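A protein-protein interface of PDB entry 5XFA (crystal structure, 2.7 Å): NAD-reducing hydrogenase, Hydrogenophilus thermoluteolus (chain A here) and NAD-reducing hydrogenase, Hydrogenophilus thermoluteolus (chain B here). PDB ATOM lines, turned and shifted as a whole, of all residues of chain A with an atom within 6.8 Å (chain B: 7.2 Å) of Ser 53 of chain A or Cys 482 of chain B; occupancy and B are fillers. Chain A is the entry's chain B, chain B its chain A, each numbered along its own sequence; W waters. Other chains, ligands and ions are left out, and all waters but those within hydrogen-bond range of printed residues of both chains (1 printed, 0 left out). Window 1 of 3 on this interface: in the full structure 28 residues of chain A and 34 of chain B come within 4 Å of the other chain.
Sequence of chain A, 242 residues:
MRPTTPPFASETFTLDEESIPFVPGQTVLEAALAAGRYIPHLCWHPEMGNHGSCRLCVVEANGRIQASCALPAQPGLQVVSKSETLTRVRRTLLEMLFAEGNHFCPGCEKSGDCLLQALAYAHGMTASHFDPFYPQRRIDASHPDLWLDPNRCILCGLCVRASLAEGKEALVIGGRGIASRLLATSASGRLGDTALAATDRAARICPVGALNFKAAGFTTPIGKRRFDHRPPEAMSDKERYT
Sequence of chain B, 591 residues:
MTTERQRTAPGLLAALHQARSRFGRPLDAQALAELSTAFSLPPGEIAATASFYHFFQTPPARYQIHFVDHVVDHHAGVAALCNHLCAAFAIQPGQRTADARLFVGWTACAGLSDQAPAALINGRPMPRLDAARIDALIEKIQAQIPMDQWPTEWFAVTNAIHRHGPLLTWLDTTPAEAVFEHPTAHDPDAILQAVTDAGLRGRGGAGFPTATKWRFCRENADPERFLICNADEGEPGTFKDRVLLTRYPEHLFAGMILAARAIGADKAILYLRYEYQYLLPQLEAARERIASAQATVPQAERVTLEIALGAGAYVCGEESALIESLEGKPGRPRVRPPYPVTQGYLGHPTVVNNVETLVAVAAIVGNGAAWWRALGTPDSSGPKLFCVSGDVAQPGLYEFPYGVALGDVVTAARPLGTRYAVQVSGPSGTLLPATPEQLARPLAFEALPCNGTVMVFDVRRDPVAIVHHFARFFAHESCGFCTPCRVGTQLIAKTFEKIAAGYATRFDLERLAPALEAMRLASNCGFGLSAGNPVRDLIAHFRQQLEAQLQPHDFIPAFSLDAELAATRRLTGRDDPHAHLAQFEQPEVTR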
ATOM      1  N   CYS A  43     -15.728  22.822 -26.837  1.00  0.00           N
ATOM      2  CA  CYS A  43     -15.935  24.181 -26.352  1.00  0.00           C
ATOM      3  C   CYS A  43     -14.661  24.960 -26.153  1.00  0.00           C
ATOM      4  O   CYS A  43     -14.708  26.176 -26.086  1.00  0.00           O
ATOM      5  CB  CYS A  43     -16.760  24.169 -25.065  1.00  0.00           C
ATOM      6  SG  CYS A  43     -15.940  23.487 -23.626  1.00  0.00           S
ATOM      7  N   HIS A  51     -14.033  26.618 -21.383  1.00  0.00           N
ATOM      8  CA  HIS A  51     -15.422  26.886 -21.033  1.00  0.00           C
ATOM      9  C   HIS A  51     -15.906  25.809 -20.091  1.00  0.00           C
ATOM     10  O   HIS A  51     -16.425  26.118 -19.046  1.00  0.00           O
ATOM     11  CB  HIS A  51     -16.292  26.927 -22.313  1.00  0.00           C
ATOM     12  CG  HIS A  51     -17.734  27.266 -22.069  1.00  0.00           C
ATOM     13  ND1 HIS A  51     -18.272  28.489 -22.377  1.00  0.00           N
ATOM     14  CD2 HIS A  51     -18.750  26.535 -21.558  1.00  0.00           C
ATOM     15  CE1 HIS A  51     -19.554  28.504 -22.059  1.00  0.00           C
ATOM     16  NE2 HIS A  51     -19.870  27.330 -21.561  1.00  0.00           N
ATOM     17  N   GLY A  52     -15.760  24.543 -20.487  1.00  0.00           N
ATOM     18  CA  GLY A  52     -16.018  23.411 -19.585  1.00  0.00           C
ATOM     19  C   GLY A  52     -17.402  22.776 -19.623  1.00  0.00           C
ATOM     20  O   GLY A  52     -17.852  22.221 -18.612  1.00  0.00           O
ATOM     21  N   SER A  53     -18.063  22.822 -20.790  1.00  0.00           N
ATOM     22  CA  SER A  53     -19.458  22.385 -20.937  1.00  0.00           C
ATOM     23  C   SER A  53     -19.546  21.108 -21.727  1.00  0.00           C
ATOM     24  O   SER A  53     -20.422  20.281 -21.463  1.00  0.00           O
ATOM     25  CB  SER A  53     -20.313  23.466 -21.603  1.00  0.00           C
ATOM     26  OG  SER A  53     -19.744  23.888 -22.838  1.00  0.00           O
ATOM     27  N   CYS A  54     -18.659  20.924 -22.701  1.00  0.00           N
ATOM     28  CA  CYS A  54     -18.804  19.771 -23.606  1.00  0.00           C
ATOM     29  C   CYS A  54     -18.441  18.450 -22.905  1.00  0.00           C
ATOM     30  O   CYS A  54     -19.215  17.489 -22.947  1.00  0.00           O
ATOM     31  CB  CYS A  54     -18.024  19.967 -24.920  1.00  0.00           C
ATOM     32  SG  CYS A  54     -16.227  19.788 -24.910  1.00  0.00           S
ATOM     33  N   ARG A  55     -17.283  18.470 -22.230  1.00  0.00           N
ATOM     34  CA  ARG A  55     -16.706  17.385 -21.413  1.00  0.00           C
ATOM     35  C   ARG A  55     -15.949  16.382 -22.237  1.00  0.00           C
ATOM     36  O   ARG A  55     -15.588  15.337 -21.741  1.00  0.00           O
ATOM     37  CB  ARG A  55     -17.746  16.685 -20.526  1.00  0.00           C
ATOM     38  CG  ARG A  55     -18.658  17.621 -19.747  1.00  0.00           C
ATOM     39  CD  ARG A  55     -17.924  18.761 -19.053  1.00  0.00           C
ATOM     40  NE  ARG A  55     -17.004  18.248 -18.053  1.00  0.00           N
ATOM     41  CZ  ARG A  55     -16.330  19.012 -17.202  1.00  0.00           C
ATOM     42  NH1 ARG A  55     -16.449  20.329 -17.243  1.00  0.00           N
ATOM     43  NH2 ARG A  55     -15.523  18.463 -16.317  1.00  0.00           N
ATOM     44  N   LEU A  56     -15.707  16.687 -23.499  1.00  0.00           N
ATOM     45  CA  LEU A  56     -15.034  15.726 -24.379  1.00  0.00           C
ATOM     46  C   LEU A  56     -13.565  15.658 -24.037  1.00  0.00           C
ATOM     47  O   LEU A  56     -12.906  14.666 -24.314  1.00  0.00           O
ATOM     48  CB  LEU A  56     -15.174  16.141 -25.842  1.00  0.00           C
ATOM     49  CG  LEU A  56     -16.466  15.809 -26.582  1.00  0.00           C
ATOM     50  CD1 LEU A  56     -16.561  14.311 -26.822  1.00  0.00           C
ATOM     51  CD2 LEU A  56     -17.689  16.314 -25.842  1.00  0.00           C
ATOM     52  N   CYS A  69      -9.303  20.870 -19.976  1.00  0.00           N
ATOM     53  CA  CYS A  69      -9.351  22.301 -20.320  1.00  0.00           C
ATOM     54  C   CYS A  69      -9.305  23.198 -19.064  1.00  0.00           C
ATOM     55  O   CYS A  69      -9.053  24.401 -19.141  1.00  0.00           O
ATOM     56  CB  CYS A  69     -10.568  22.627 -21.219  1.00  0.00           C
ATOM     57  SG  CYS A  69     -12.275  22.365 -20.608  1.00  0.00           S
ATOM     58  N   LEU A  93     -21.081  10.895 -24.389  1.00  0.00           N
ATOM     59  CA  LEU A  93     -21.385  12.328 -24.446  1.00  0.00           C
ATOM     60  C   LEU A  93     -21.825  12.749 -25.861  1.00  0.00           C
ATOM     61  O   LEU A  93     -22.729  13.573 -26.038  1.00  0.00           O
ATOM     62  CB  LEU A  93     -20.177  13.157 -24.009  1.00  0.00           C
ATOM     63  CG  LEU A  93     -19.697  12.965 -22.572  1.00  0.00           C
ATOM     64  CD1 LEU A  93     -18.303  13.543 -22.372  1.00  0.00           C
ATOM     65  CD2 LEU A  93     -20.694  13.583 -21.616  1.00  0.00           C
ATOM     66  N   LEU A  97     -25.480  14.654 -26.888  1.00  0.00           N
ATOM     67  CA  LEU A  97     -25.626  15.905 -27.620  1.00  0.00           C
ATOM     68  C   LEU A  97     -26.475  15.715 -28.859  1.00  0.00           C
ATOM     69  O   LEU A  97     -27.326  16.549 -29.159  1.00  0.00           O
ATOM     70  CB  LEU A  97     -24.248  16.469 -27.964  1.00  0.00           C
ATOM     71  CG  LEU A  97     -23.531  17.059 -26.731  1.00  0.00           C
ATOM     72  CD1 LEU A  97     -22.119  17.529 -27.071  1.00  0.00           C
ATOM     73  CD2 LEU A  97     -24.330  18.198 -26.111  1.00  0.00           C
ATOM     74  N   ILE A 154     -25.199  23.543 -29.183  1.00  0.00           N
ATOM     75  CA  ILE A 154     -24.673  22.627 -28.175  1.00  0.00           C
ATOM     76  C   ILE A 154     -24.210  23.353 -26.934  1.00  0.00           C
ATOM     77  O   ILE A 154     -23.535  22.759 -26.095  1.00  0.00           O
ATOM     78  CB  ILE A 154     -23.477  21.845 -28.717  1.00  0.00           C
ATOM     79  CG1 ILE A 154     -22.342  22.814 -29.120  1.00  0.00           C
ATOM     80  CG2 ILE A 154     -23.916  20.965 -29.891  1.00  0.00           C
ATOM     81  CD1 ILE A 154     -21.006  22.146 -29.371  1.00  0.00           C
ATOM     82  N   LEU A 155     -24.533  24.649 -26.849  1.00  0.00           N
ATOM     83  CA  LEU A 155     -24.199  25.464 -25.699  1.00  0.00           C
ATOM     84  C   LEU A 155     -22.712  25.395 -25.373  1.00  0.00           C
ATOM     85  O   LEU A 155     -22.332  25.195 -24.220  1.00  0.00           O
ATOM     86  CB  LEU A 155     -25.018  25.028 -24.490  1.00  0.00           C
ATOM     87  CG  LEU A 155     -26.520  25.039 -24.763  1.00  0.00           C
ATOM     88  CD1 LEU A 155     -27.270  24.114 -23.811  1.00  0.00           C
ATOM     89  CD2 LEU A 155     -27.052  26.472 -24.681  1.00  0.00           C
ATOM     90  N   CYS A 156     -21.878  25.558 -26.406  1.00  0.00           N
ATOM     91  CA  CYS A 156     -20.437  25.694 -26.220  1.00  0.00           C
ATOM     92  C   CYS A 156     -20.115  27.064 -25.664  1.00  0.00           C
ATOM     93  O   CYS A 156     -19.161  27.238 -24.940  1.00  0.00           O
ATOM     94  CB  CYS A 156     -19.704  25.506 -27.537  1.00  0.00           C
ATOM     95  SG  CYS A 156     -20.007  26.767 -28.802  1.00  0.00           S
ATOM     96  N   GLY A 157     -20.921  28.048 -26.027  1.00  0.00           N
ATOM     97  CA  GLY A 157     -20.761  29.386 -25.525  1.00  0.00           C
ATOM     98  C   GLY A 157     -19.706  30.182 -26.268  1.00  0.00           C
ATOM     99  O   GLY A 157     -19.340  31.264 -25.812  1.00  0.00           O
ATOM    100  N   ARG A 161     -18.859  34.262 -25.742  1.00  0.00           N
ATOM    101  CA  ARG A 161     -17.515  34.764 -25.397  1.00  0.00           C
ATOM    102  C   ARG A 161     -16.976  35.677 -26.469  1.00  0.00           C
ATOM    103  O   ARG A 161     -16.498  36.757 -26.192  1.00  0.00           O
ATOM    104  CB  ARG A 161     -16.521  33.628 -25.173  1.00  0.00           C
ATOM    105  CG  ARG A 161     -17.063  32.518 -24.290  1.00  0.00           C
ATOM    106  CD  ARG A 161     -16.020  31.765 -23.476  1.00  0.00           C
ATOM    107  NE  ARG A 161     -15.236  30.722 -24.168  1.00  0.00           N
ATOM    108  CZ  ARG A 161     -15.721  29.640 -24.780  1.00  0.00           C
ATOM    109  NH1 ARG A 161     -17.017  29.445 -24.899  1.00  0.00           N
ATOM    110  NH2 ARG A 161     -14.893  28.760 -25.317  1.00  0.00           N
ATOM    111  N   VAL B 335     -15.856  27.216 -13.191  1.00  0.00           N
ATOM    112  CA  VAL B 335     -14.804  26.285 -13.564  1.00  0.00           C
ATOM    113  C   VAL B 335     -13.670  26.525 -12.584  1.00  0.00           C
ATOM    114  O   VAL B 335     -13.016  27.562 -12.635  1.00  0.00           O
ATOM    115  CB  VAL B 335     -14.232  26.492 -14.984  1.00  0.00           C
ATOM    116  CG1 VAL B 335     -14.324  25.177 -15.757  1.00  0.00           C
ATOM    117  CG2 VAL B 335     -14.919  27.635 -15.732  1.00  0.00           C
ATOM    118  N   SER B 478     -30.965  20.680 -11.815  1.00  0.00           N
ATOM    119  CA  SER B 478     -29.716  20.766 -12.585  1.00  0.00           C
ATOM    120  C   SER B 478     -29.512  22.114 -13.244  1.00  0.00           C
ATOM    121  O   SER B 478     -30.432  22.646 -13.847  1.00  0.00           O
ATOM    122  CB  SER B 478     -29.689  19.724 -13.698  1.00  0.00           C
ATOM    123  OG  SER B 478     -28.516  19.883 -14.473  1.00  0.00           O
ATOM    124  N   CYS B 479     -28.293  22.645 -13.174  1.00  0.00           N
ATOM    125  CA  CYS B 479     -28.045  23.982 -13.715  1.00  0.00           C
ATOM    126  C   CYS B 479     -27.959  24.020 -15.248  1.00  0.00           C
ATOM    127  O   CYS B 479     -27.980  25.091 -15.817  1.00  0.00           O
ATOM    128  CB  CYS B 479     -26.810  24.625 -13.071  1.00  0.00           C
ATOM    129  SG  CYS B 479     -25.253  24.408 -13.964  1.00  0.00           S
ATOM    130  N   GLY B 480     -27.870  22.866 -15.899  1.00  0.00           N
ATOM    131  CA  GLY B 480     -27.929  22.780 -17.372  1.00  0.00           C
ATOM    132  C   GLY B 480     -26.644  23.203 -18.089  1.00  0.00           C
ATOM    133  O   GLY B 480     -26.618  23.375 -19.313  1.00  0.00           O
ATOM    134  N   PHE B 481     -25.561  23.362 -17.338  1.00  0.00           N
ATOM    135  CA  PHE B 481     -24.327  23.906 -17.895  1.00  0.00           C
ATOM    136  C   PHE B 481     -23.527  22.853 -18.680  1.00  0.00           C
ATOM    137  O   PHE B 481     -22.881  23.187 -19.666  1.00  0.00           O
ATOM    138  CB  PHE B 481     -23.429  24.567 -16.784  1.00  0.00           C
ATOM    139  CG  PHE B 481     -22.076  24.915 -17.275  1.00  0.00           C
ATOM    140  CD1 PHE B 481     -21.917  25.937 -18.200  1.00  0.00           C
ATOM    141  CD2 PHE B 481     -20.978  24.173 -16.918  1.00  0.00           C
ATOM    142  CE1 PHE B 481     -20.655  26.252 -18.726  1.00  0.00           C
ATOM    143  CE2 PHE B 481     -19.710  24.475 -17.432  1.00  0.00           C
ATOM    144  CZ  PHE B 481     -19.543  25.518 -18.339  1.00  0.00           C
ATOM    145  N   CYS B 482     -23.501  21.610 -18.197  1.00  0.00           N
ATOM    146  CA  CYS B 482     -22.554  20.618 -18.732  1.00  0.00           C
ATOM    147  C   CYS B 482     -23.235  19.355 -19.252  1.00  0.00           C
ATOM    148  O   CYS B 482     -24.258  18.917 -18.757  1.00  0.00           O
ATOM    149  CB  CYS B 482     -21.427  20.331 -17.704  1.00  0.00           C
ATOM    150  SG  CYS B 482     -21.695  19.210 -16.293  1.00  0.00           S
ATOM    151  N   THR B 483     -22.677  18.799 -20.299  1.00  0.00           N
ATOM    152  CA  THR B 483     -23.372  17.749 -21.077  1.00  0.00           C
ATOM    153  C   THR B 483     -23.955  16.566 -20.306  1.00  0.00           C
ATOM    154  O   THR B 483     -25.154  16.343 -20.378  1.00  0.00           O
ATOM    155  CB  THR B 483     -22.443  17.191 -22.133  1.00  0.00           C
ATOM    156  OG1 THR B 483     -21.878  18.277 -22.872  1.00  0.00           O
ATOM    157  CG2 THR B 483     -23.197  16.280 -23.046  1.00  0.00           C
ATOM    158  N   PRO B 484     -23.123  15.823 -19.541  1.00  0.00           N
ATOM    159  CA  PRO B 484     -23.625  14.603 -18.895  1.00  0.00           C
ATOM    160  C   PRO B 484     -24.696  14.849 -17.838  1.00  0.00           C
ATOM    161  O   PRO B 484     -25.542  14.001 -17.594  1.00  0.00           O
ATOM    162  CB  PRO B 484     -22.377  14.024 -18.232  1.00  0.00           C
ATOM    163  CG  PRO B 484     -21.566  15.214 -17.911  1.00  0.00           C
ATOM    164  CD  PRO B 484     -21.747  16.119 -19.097  1.00  0.00           C
ATOM    165  N   CYS B 485     -24.666  16.009 -17.216  1.00  0.00           N
ATOM    166  CA  CYS B 485     -25.602  16.304 -16.145  1.00  0.00           C
ATOM    167  C   CYS B 485     -26.858  16.924 -16.708  1.00  0.00           C
ATOM    168  O   CYS B 485     -27.955  16.577 -16.294  1.00  0.00           O
ATOM    169  CB  CYS B 485     -24.950  17.237 -15.135  1.00  0.00           C
ATOM    170  SG  CYS B 485     -26.123  17.780 -13.888  1.00  0.00           S
ATOM    171  N   ARG B 486     -26.700  17.852 -17.647  1.00  0.00           N
ATOM    172  CA  ARG B 486     -27.852  18.538 -18.244  1.00  0.00           C
ATOM    173  C   ARG B 486     -28.792  17.540 -18.847  1.00  0.00           C
ATOM    174  O   ARG B 486     -29.975  17.537 -18.527  1.00  0.00           O
ATOM    175  CB  ARG B 486     -27.416  19.505 -19.351  1.00  0.00           C
ATOM    176  CG  ARG B 486     -28.567  20.123 -20.141  1.00  0.00           C
ATOM    177  CD  ARG B 486     -28.090  21.261 -21.032  1.00  0.00           C
ATOM    178  NE  ARG B 486     -27.322  20.801 -22.183  1.00  0.00           N
ATOM    179  CZ  ARG B 486     -25.993  20.825 -22.311  1.00  0.00           C
ATOM    180  NH1 ARG B 486     -25.187  21.285 -21.359  1.00  0.00           N
ATOM    181  NH2 ARG B 486     -25.453  20.355 -23.429  1.00  0.00           N
ATOM    182  N   VAL B 487     -28.235  16.685 -19.700  1.00  0.00           N
ATOM    183  CA  VAL B 487     -28.985  15.660 -20.416  1.00  0.00           C
ATOM    184  C   VAL B 487     -29.255  14.464 -19.523  1.00  0.00           C
ATOM    185  O   VAL B 487     -30.363  13.937 -19.501  1.00  0.00           O
ATOM    186  CB  VAL B 487     -28.204  15.163 -21.652  1.00  0.00           C
ATOM    187  CG1 VAL B 487     -28.943  14.037 -22.368  1.00  0.00           C
ATOM    188  CG2 VAL B 487     -27.924  16.308 -22.619  1.00  0.00           C
ATOM    189  N   GLY B 488     -28.233  14.010 -18.810  1.00  0.00           N
ATOM    190  CA  GLY B 488     -28.284  12.696 -18.167  1.00  0.00           C
ATOM    191  C   GLY B 488     -29.272  12.631 -17.025  1.00  0.00           C
ATOM    192  O   GLY B 488     -29.913  11.607 -16.799  1.00  0.00           O
ATOM    193  N   ALA B 522     -17.643  12.433 -15.594  1.00  0.00           N
ATOM    194  CA  ALA B 522     -17.397  13.616 -16.453  1.00  0.00           C
ATOM    195  C   ALA B 522     -18.118  14.921 -16.047  1.00  0.00           C
ATOM    196  O   ALA B 522     -17.755  15.969 -16.549  1.00  0.00           O
ATOM    197  CB  ALA B 522     -17.709  13.280 -17.914  1.00  0.00           C
ATOM    198  N   SER B 523     -19.107  14.871 -15.163  1.00  0.00           N
ATOM    199  CA  SER B 523     -19.758  16.100 -14.677  1.00  0.00           C
ATOM    200  C   SER B 523     -18.760  17.175 -14.246  1.00  0.00           C
ATOM    201  O   SER B 523     -17.642  16.879 -13.859  1.00  0.00           O
ATOM    202  CB  SER B 523     -20.683  15.806 -13.479  1.00  0.00           C
ATOM    203  OG  SER B 523     -21.923  15.306 -13.911  1.00  0.00           O
ATOM    204  N   ASN B 524     -19.197  18.422 -14.257  1.00  0.00           N
ATOM    205  CA  ASN B 524     -18.328  19.542 -13.879  1.00  0.00           C
ATOM    206  C   ASN B 524     -18.362  19.874 -12.384  1.00  0.00           C
ATOM    207  O   ASN B 524     -17.427  20.441 -11.876  1.00  0.00           O
ATOM    208  CB  ASN B 524     -18.707  20.785 -14.696  1.00  0.00           C
ATOM    209  CG  ASN B 524     -18.094  22.080 -14.154  1.00  0.00           C
ATOM    210  OD1 ASN B 524     -16.903  22.328 -14.283  1.00  0.00           O
ATOM    211  ND2 ASN B 524     -18.922  22.908 -13.546  1.00  0.00           N
ATOM    212  N   CYS B 525     -19.452  19.542 -11.699  1.00  0.00           N
ATOM    213  CA  CYS B 525     -19.544  19.756 -10.268  1.00  0.00           C
ATOM    214  C   CYS B 525     -20.147  18.553  -9.519  1.00  0.00           C
ATOM    215  O   CYS B 525     -20.537  17.572 -10.120  1.00  0.00           O
ATOM    216  CB  CYS B 525     -20.332  21.031 -10.002  1.00  0.00           C
ATOM    217  SG  CYS B 525     -22.118  20.826  -9.959  1.00  0.00           S
ATOM    218  N   GLY B 528     -23.790  16.820 -10.362  1.00  0.00           N
ATOM    219  CA  GLY B 528     -23.843  15.793 -11.404  1.00  0.00           C
ATOM    220  C   GLY B 528     -23.229  14.462 -10.995  1.00  0.00           C
ATOM    221  O   GLY B 528     -23.584  13.407 -11.526  1.00  0.00           O
HETATM  222  O   HOH W   1     -22.913  21.017 -23.039  1.00  0.00           O
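O of Ala 522 of chain B sits at hydrogen-bond distance from NE of Arg 55 of chain A.
The backbone carbonyl oxygen (O) of Cys 54 of chain A is in hydrogen-bond range of the side-chain hydroxyl (OG1) of Thr 483 of chain B.
The side-chain hydroxyl (OG1) of Thr 483 of chain B sits at hydrogen-bond distance from the backbone carbonyl oxygen (O) of Ser 53 of chain A, at 2.8 Å.
NH1 of Arg 161 of chain A lies within hydrogen-bond range of ND1 of His 51 of chain A, at 3.0 Å.
The backbone NH of Ser 53 of chain A lies close to the side-chain sulfur of Cys 43 of chain A (3.6 Å).
The backbone NH (N) of Asn 524 of chain B lies close to the side-chain sulfur (SG) of Cys 482 of chain B (3.3 Å).
The side-chain sulfur of Cys 479 of chain B sits close to the backbone NH of Phe 481 of chain B (3.5 Å).
The backbone NH (N) of Gly 52 of chain A sits close to the side-chain sulfur (SG) of Cys 43 of chain A, at 3.3 Å.
The backbone carbonyl oxygen (O) of Gly 528 of chain B lies close to the side-chain hydroxyl (OG) of Ser 523 of chain B, at 3.5 Å.
Among the printed residues, merely in contact across the chains: His 51 of chain A with Phe 481 of chain B (3.1 Å), Gly 52 of chain A with Phe 481 of chain B (3.2 Å), Ser 53 of chain A with Phe 481 of chain B (3.2 Å), Arg 55 of chain A with Asn 524 of chain B (3.4 Å), Ser 53 of chain A with Cys 482 of chain B (3.5 Å), Arg 55 of chain A with Pro 484 of chain B (3.5 Å), Arg 55 of chain A with Ser 523 of chain B (3.6 Å), Leu 97 of chain A with Arg 486 of chain B (3.6 Å), Leu 155 of chain A with Arg 486 of chain B (3.7 Å), Leu 93 of chain A with Pro 484 of chain B (3.7 Å), Leu 97 of chain A with Thr 483 of chain B (3.8 Å), His 51 of chain A with Val 335 of chain B (3.9 Å) and Leu 93 of chain A with Thr 483 of chain B (3.9 Å).
Cys 482 of chain B touches just one residue of chain A: Ser 53 (3.5 Å).
Of chain B, only Phe 481 (3.2 Å) comes within 4 Å of Gly 52 of chain A.
Printed residues of chain B within 4 Å of His 51 of chain A: Val 335 (3.9 Å) and Phe 481 (3.1 Å).
Printed residues of chain B within 4 Å of Leu 97 of chain A: Thr 483 and Arg 486.
Of the printed residues of chain B, Cys 54 of chain A touches Thr 483.
Of the printed residues of chain A, Ala 522 of chain B touches Arg 55 (2.8 Å).
The nearest residue of chain B that does not touch Ser 53 of chain A is Arg 486 of chain B (4.9 Å).
The nearest residue of chain A that does not touch Cys 482 of chain B is Arg 55 of chain A (4.1 Å).
Of the 15 printed residues of chain A, 8 touch a printed residue of chain B.
Of the 17 printed residues of chain B, 9 touch a printed residue of chain A.
Printed residues of chain B that touch a printed residue of chain A: Val 335, Phe 481, Cys 482, Thr 483, Pro 484, Arg 486, Ala 522, Ser 523 and Asn 524.
Among the printed residues, 16 pairs touch across the chains.
Water W1 lies within hydrogen-bond range of NH2 of Arg 486 of chain B (2.7 Å), OG1 of Thr 483 of chain B (2.9 Å) and O of Ser 53 of chain A (3.0 Å).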
